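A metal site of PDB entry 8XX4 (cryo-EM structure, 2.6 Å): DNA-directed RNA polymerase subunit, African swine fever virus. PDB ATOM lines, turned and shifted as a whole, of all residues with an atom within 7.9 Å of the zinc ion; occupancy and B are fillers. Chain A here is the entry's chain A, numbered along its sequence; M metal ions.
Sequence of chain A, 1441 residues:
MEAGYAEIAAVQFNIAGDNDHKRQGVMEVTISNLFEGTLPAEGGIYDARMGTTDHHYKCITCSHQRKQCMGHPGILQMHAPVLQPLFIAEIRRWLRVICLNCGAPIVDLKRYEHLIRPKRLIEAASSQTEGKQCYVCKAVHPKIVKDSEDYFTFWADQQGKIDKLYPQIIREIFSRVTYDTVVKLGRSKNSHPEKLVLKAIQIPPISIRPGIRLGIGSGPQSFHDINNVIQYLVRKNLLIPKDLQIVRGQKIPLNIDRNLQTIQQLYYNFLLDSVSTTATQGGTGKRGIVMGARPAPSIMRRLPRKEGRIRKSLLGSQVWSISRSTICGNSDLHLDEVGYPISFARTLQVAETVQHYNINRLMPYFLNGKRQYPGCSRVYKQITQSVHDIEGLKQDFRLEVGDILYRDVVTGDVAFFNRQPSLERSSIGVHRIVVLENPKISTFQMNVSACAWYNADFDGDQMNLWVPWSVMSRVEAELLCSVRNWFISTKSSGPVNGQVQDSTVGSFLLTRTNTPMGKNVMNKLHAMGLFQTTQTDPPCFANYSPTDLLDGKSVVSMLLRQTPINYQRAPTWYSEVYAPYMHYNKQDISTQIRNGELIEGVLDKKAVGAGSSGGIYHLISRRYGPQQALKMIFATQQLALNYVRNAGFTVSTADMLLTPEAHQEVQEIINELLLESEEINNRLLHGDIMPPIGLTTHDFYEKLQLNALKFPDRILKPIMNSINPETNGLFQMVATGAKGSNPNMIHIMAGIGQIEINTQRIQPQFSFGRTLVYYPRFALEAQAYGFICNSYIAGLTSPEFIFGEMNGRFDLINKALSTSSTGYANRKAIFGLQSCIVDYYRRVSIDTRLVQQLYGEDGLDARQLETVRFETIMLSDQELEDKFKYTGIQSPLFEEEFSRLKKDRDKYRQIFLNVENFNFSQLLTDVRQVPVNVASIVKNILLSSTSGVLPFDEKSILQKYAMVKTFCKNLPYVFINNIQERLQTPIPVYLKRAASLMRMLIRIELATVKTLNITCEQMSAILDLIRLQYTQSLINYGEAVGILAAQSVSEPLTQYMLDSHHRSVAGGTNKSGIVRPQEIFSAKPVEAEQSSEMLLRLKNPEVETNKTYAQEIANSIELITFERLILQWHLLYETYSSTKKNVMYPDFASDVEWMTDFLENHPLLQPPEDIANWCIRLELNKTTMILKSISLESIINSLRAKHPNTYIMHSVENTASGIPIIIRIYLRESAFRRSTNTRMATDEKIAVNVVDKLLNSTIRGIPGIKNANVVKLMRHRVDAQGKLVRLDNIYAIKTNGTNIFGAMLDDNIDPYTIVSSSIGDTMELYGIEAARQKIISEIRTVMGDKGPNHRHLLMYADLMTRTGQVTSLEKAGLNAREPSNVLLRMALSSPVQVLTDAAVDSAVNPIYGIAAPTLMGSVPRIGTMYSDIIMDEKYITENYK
Within 4 Å of the zinc ion: Cys 99, Cys 102, Cys 134 and Cys 137. The nearest printed residue that does not touch the zinc ion is Asn 101 (4.3 Å).
The side-chain sulfur (SG) of Cys 134 sits close to the backbone NH (N) of Val 136 (3.7 Å). O of Ala 104 is in hydrogen-bond range of N of Cys 99 (2.7 Å). O of Cys 134 sits at hydrogen-bond distance from NZ of Lys 138 (3.1 Å). The backbone NH (N) of Cys 134 sits at hydrogen-bond distance from the backbone carbonyl oxygen (O) of Ala 139, 2.8 Å away. N of Asn 101 sits close to SG of Cys 99 (3.2 Å).
The zinc ion is bound by SG of Cys 102 (2.3 Å), SG of Cys 137 (2.3 Å), SG of Cys 134 (2.3 Å) and SG of Cys 99 (2.3 Å). The zinc ion has four donor atoms within binding distance.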
ATOM      1  N   ILE A  98      19.039   6.348 -21.004  1.00  0.00           N
ATOM      2  CA  ILE A  98      19.911   5.578 -20.133  1.00  0.00           C
ATOM      3  C   ILE A  98      21.050   6.471 -19.673  1.00  0.00           C
ATOM      4  O   ILE A  98      21.430   7.426 -20.363  1.00  0.00           O
ATOM      5  CB  ILE A  98      20.455   4.326 -20.851  1.00  0.00           C
ATOM      6  CG1 ILE A  98      21.081   4.741 -22.170  1.00  0.00           C
ATOM      7  CG2 ILE A  98      19.350   3.316 -21.077  1.00  0.00           C
ATOM      8  CD1 ILE A  98      22.365   4.041 -22.476  1.00  0.00           C
ATOM      9  N   CYS A  99      21.603   6.154 -18.508  1.00  0.00           N
ATOM     10  CA  CYS A  99      22.725   6.907 -17.968  1.00  0.00           C
ATOM     11  C   CYS A  99      23.983   6.576 -18.751  1.00  0.00           C
ATOM     12  O   CYS A  99      24.303   5.404 -18.968  1.00  0.00           O
ATOM     13  CB  CYS A  99      22.921   6.585 -16.492  1.00  0.00           C
ATOM     14  SG  CYS A  99      24.636   6.713 -15.956  1.00  0.00           S
ATOM     15  N   LEU A 100      24.712   7.613 -19.177  1.00  0.00           N
ATOM     16  CA  LEU A 100      25.924   7.401 -19.958  1.00  0.00           C
ATOM     17  C   LEU A 100      27.133   7.143 -19.078  1.00  0.00           C
ATOM     18  O   LEU A 100      28.212   7.674 -19.329  1.00  0.00           O
ATOM     19  CB  LEU A 100      26.174   8.615 -20.853  1.00  0.00           C
ATOM     20  CG  LEU A 100      25.096   9.176 -21.791  1.00  0.00           C
ATOM     21  CD1 LEU A 100      24.129  10.067 -21.056  1.00  0.00           C
ATOM     22  CD2 LEU A 100      25.751   9.944 -22.915  1.00  0.00           C
ATOM     23  N   ASN A 101      26.986   6.305 -18.059  1.00  0.00           N
ATOM     24  CA  ASN A 101      28.117   5.832 -17.274  1.00  0.00           C
ATOM     25  C   ASN A 101      28.038   4.357 -16.903  1.00  0.00           C
ATOM     26  O   ASN A 101      29.081   3.742 -16.676  1.00  0.00           O
ATOM     27  CB  ASN A 101      28.263   6.652 -15.992  1.00  0.00           C
ATOM     28  CG  ASN A 101      28.829   8.029 -16.236  1.00  0.00           C
ATOM     29  OD1 ASN A 101      28.089   8.984 -16.489  1.00  0.00           O
ATOM     30  ND2 ASN A 101      30.145   8.145 -16.170  1.00  0.00           N
ATOM     31  N   CYS A 102      26.838   3.765 -16.825  1.00  0.00           N
ATOM     32  CA  CYS A 102      26.685   2.369 -16.444  1.00  0.00           C
ATOM     33  C   CYS A 102      25.607   1.677 -17.264  1.00  0.00           C
ATOM     34  O   CYS A 102      25.295   0.509 -16.976  1.00  0.00           O
ATOM     35  CB  CYS A 102      26.361   2.240 -14.956  1.00  0.00           C
ATOM     36  SG  CYS A 102      24.930   3.216 -14.428  1.00  0.00           S
ATOM     37  N   GLY A 103      25.022   2.343 -18.248  1.00  0.00           N
ATOM     38  CA  GLY A 103      23.934   1.764 -19.007  1.00  0.00           C
ATOM     39  C   GLY A 103      22.686   1.522 -18.187  1.00  0.00           C
ATOM     40  O   GLY A 103      21.959   0.550 -18.448  1.00  0.00           O
ATOM     41  N   ALA A 104      22.415   2.362 -17.205  1.00  0.00           N
ATOM     42  CA  ALA A 104      21.224   2.116 -16.429  1.00  0.00           C
ATOM     43  C   ALA A 104      20.078   3.003 -16.905  1.00  0.00           C
ATOM     44  O   ALA A 104      20.311   4.146 -17.304  1.00  0.00           O
ATOM     45  CB  ALA A 104      21.474   2.381 -14.936  1.00  0.00           C
ATOM     46  N   PRO A 105      18.849   2.493 -16.871  1.00  0.00           N
ATOM     47  CA  PRO A 105      17.716   3.274 -17.378  1.00  0.00           C
ATOM     48  C   PRO A 105      17.243   4.316 -16.391  1.00  0.00           C
ATOM     49  O   PRO A 105      16.348   4.042 -15.589  1.00  0.00           O
ATOM     50  CB  PRO A 105      16.644   2.205 -17.606  1.00  0.00           C
ATOM     51  CG  PRO A 105      16.975   1.110 -16.654  1.00  0.00           C
ATOM     52  CD  PRO A 105      18.427   1.223 -16.270  1.00  0.00           C
ATOM     53  N   ILE A 106      17.805   5.517 -16.427  1.00  0.00           N
ATOM     54  CA  ILE A 106      17.394   6.519 -15.457  1.00  0.00           C
ATOM     55  C   ILE A 106      16.080   7.130 -15.938  1.00  0.00           C
ATOM     56  O   ILE A 106      16.040   8.234 -16.505  1.00  0.00           O
ATOM     57  CB  ILE A 106      18.486   7.578 -15.239  1.00  0.00           C
ATOM     58  CG1 ILE A 106      18.942   8.174 -16.560  1.00  0.00           C
ATOM     59  CG2 ILE A 106      19.667   6.970 -14.534  1.00  0.00           C
ATOM     60  CD1 ILE A 106      19.617   9.465 -16.377  1.00  0.00           C
ATOM     61  N   GLN A 133      19.569  12.419 -11.643  1.00  0.00           N
ATOM     62  CA  GLN A 133      20.513  11.620 -10.894  1.00  0.00           C
ATOM     63  C   GLN A 133      20.326  10.151 -11.221  1.00  0.00           C
ATOM     64  O   GLN A 133      19.195   9.670 -11.333  1.00  0.00           O
ATOM     65  CB  GLN A 133      20.342  11.860  -9.397  1.00  0.00           C
ATOM     66  CG  GLN A 133      21.209  11.001  -8.508  1.00  0.00           C
ATOM     67  CD  GLN A 133      22.620  11.532  -8.386  1.00  0.00           C
ATOM     68  OE1 GLN A 133      23.464  11.321  -9.253  1.00  0.00           O
ATOM     69  NE2 GLN A 133      22.887  12.234  -7.284  1.00  0.00           N
ATOM     70  N   CYS A 134      21.443   9.438 -11.379  1.00  0.00           N
ATOM     71  CA  CYS A 134      21.391   8.001 -11.630  1.00  0.00           C
ATOM     72  C   CYS A 134      21.214   7.248 -10.309  1.00  0.00           C
ATOM     73  O   CYS A 134      21.173   7.837  -9.225  1.00  0.00           O
ATOM     74  CB  CYS A 134      22.648   7.555 -12.371  1.00  0.00           C
ATOM     75  SG  CYS A 134      22.666   5.809 -12.823  1.00  0.00           S
ATOM     76  N   TYR A 135      21.109   5.929 -10.405  1.00  0.00           N
ATOM     77  CA  TYR A 135      20.955   5.068  -9.239  1.00  0.00           C
ATOM     78  C   TYR A 135      22.130   4.116  -9.059  1.00  0.00           C
ATOM     79  O   TYR A 135      22.713   4.060  -7.978  1.00  0.00           O
ATOM     80  CB  TYR A 135      19.649   4.273  -9.339  1.00  0.00           C
ATOM     81  CG  TYR A 135      18.417   5.052  -8.950  1.00  0.00           C
ATOM     82  CD1 TYR A 135      18.471   6.027  -7.957  1.00  0.00           C
ATOM     83  CD2 TYR A 135      17.202   4.827  -9.575  1.00  0.00           C
ATOM     84  CE1 TYR A 135      17.350   6.745  -7.606  1.00  0.00           C
ATOM     85  CE2 TYR A 135      16.072   5.535  -9.221  1.00  0.00           C
ATOM     86  CZ  TYR A 135      16.155   6.499  -8.238  1.00  0.00           C
ATOM     87  OH  TYR A 135      15.025   7.207  -7.884  1.00  0.00           O
ATOM     88  N   VAL A 136      22.483   3.362 -10.103  1.00  0.00           N
ATOM     89  CA  VAL A 136      23.556   2.384  -9.973  1.00  0.00           C
ATOM     90  C   VAL A 136      24.887   3.084  -9.734  1.00  0.00           C
ATOM     91  O   VAL A 136      25.661   2.687  -8.856  1.00  0.00           O
ATOM     92  CB  VAL A 136      23.617   1.489 -11.234  1.00  0.00           C
ATOM     93  CG1 VAL A 136      24.883   0.653 -11.227  1.00  0.00           C
ATOM     94  CG2 VAL A 136      22.378   0.602 -11.301  1.00  0.00           C
ATOM     95  N   CYS A 137      25.166   4.143 -10.488  1.00  0.00           N
ATOM     96  CA  CYS A 137      26.426   4.854 -10.389  1.00  0.00           C
ATOM     97  C   CYS A 137      26.290   6.270  -9.855  1.00  0.00           C
ATOM     98  O   CYS A 137      27.315   6.915  -9.594  1.00  0.00           O
ATOM     99  CB  CYS A 137      27.126   4.897 -11.755  1.00  0.00           C
ATOM    100  SG  CYS A 137      26.542   6.205 -12.842  1.00  0.00           S
ATOM    101  N   LYS A 138      25.063   6.770  -9.709  1.00  0.00           N
ATOM    102  CA  LYS A 138      24.808   8.082  -9.096  1.00  0.00           C
ATOM    103  C   LYS A 138      25.538   9.192  -9.841  1.00  0.00           C
ATOM    104  O   LYS A 138      26.443   9.847  -9.318  1.00  0.00           O
ATOM    105  CB  LYS A 138      25.192   8.059  -7.608  1.00  0.00           C
ATOM    106  CG  LYS A 138      24.096   7.574  -6.670  1.00  0.00           C
ATOM    107  CD  LYS A 138      22.950   8.565  -6.594  1.00  0.00           C
ATOM    108  CE  LYS A 138      21.808   8.050  -5.749  1.00  0.00           C
ATOM    109  NZ  LYS A 138      20.479   8.490  -6.268  1.00  0.00           N
ATOM    110  N   ALA A 139      25.144   9.390 -11.097  1.00  0.00           N
ATOM    111  CA  ALA A 139      25.738  10.396 -11.966  1.00  0.00           C
ATOM    112  C   ALA A 139      24.643  11.266 -12.554  1.00  0.00           C
ATOM    113  O   ALA A 139      23.472  10.897 -12.603  1.00  0.00           O
ATOM    114  CB  ALA A 139      26.561   9.757 -13.097  1.00  0.00           C
ATOM    115  N   VAL A 140      25.051  12.449 -13.015  1.00  0.00           N
ATOM    116  CA  VAL A 140      24.123  13.414 -13.593  1.00  0.00           C
ATOM    117  C   VAL A 140      24.080  13.209 -15.102  1.00  0.00           C
ATOM    118  O   VAL A 140      25.125  13.153 -15.759  1.00  0.00           O
ATOM    119  CB  VAL A 140      24.545  14.853 -13.236  1.00  0.00           C
ATOM    120  CG1 VAL A 140      23.859  15.848 -14.164  1.00  0.00           C
ATOM    121  CG2 VAL A 140      24.206  15.154 -11.789  1.00  0.00           C
ATOM    122  N   ARG A 176      26.894  -0.999 -22.406  1.00  0.00           N
ATOM    123  CA  ARG A 176      26.616  -1.147 -20.980  1.00  0.00           C
ATOM    124  C   ARG A 176      25.157  -1.430 -20.687  1.00  0.00           C
ATOM    125  O   ARG A 176      24.835  -1.786 -19.544  1.00  0.00           O
ATOM    126  CB  ARG A 176      27.058   0.102 -20.231  1.00  0.00           C
ATOM    127  CG  ARG A 176      28.550   0.364 -20.266  1.00  0.00           C
ATOM    128  CD  ARG A 176      28.919   1.438 -19.285  1.00  0.00           C
ATOM    129  NE  ARG A 176      28.748   2.768 -19.854  1.00  0.00           N
ATOM    130  CZ  ARG A 176      29.713   3.480 -20.408  1.00  0.00           C
ATOM    131  NH1 ARG A 176      30.955   3.025 -20.482  1.00  0.00           N
ATOM    132  NH2 ARG A 176      29.434   4.686 -20.895  1.00  0.00           N
HETATM  133 ZN    ZN M   1      24.656   5.474 -13.984  1.00  0.00          ZN
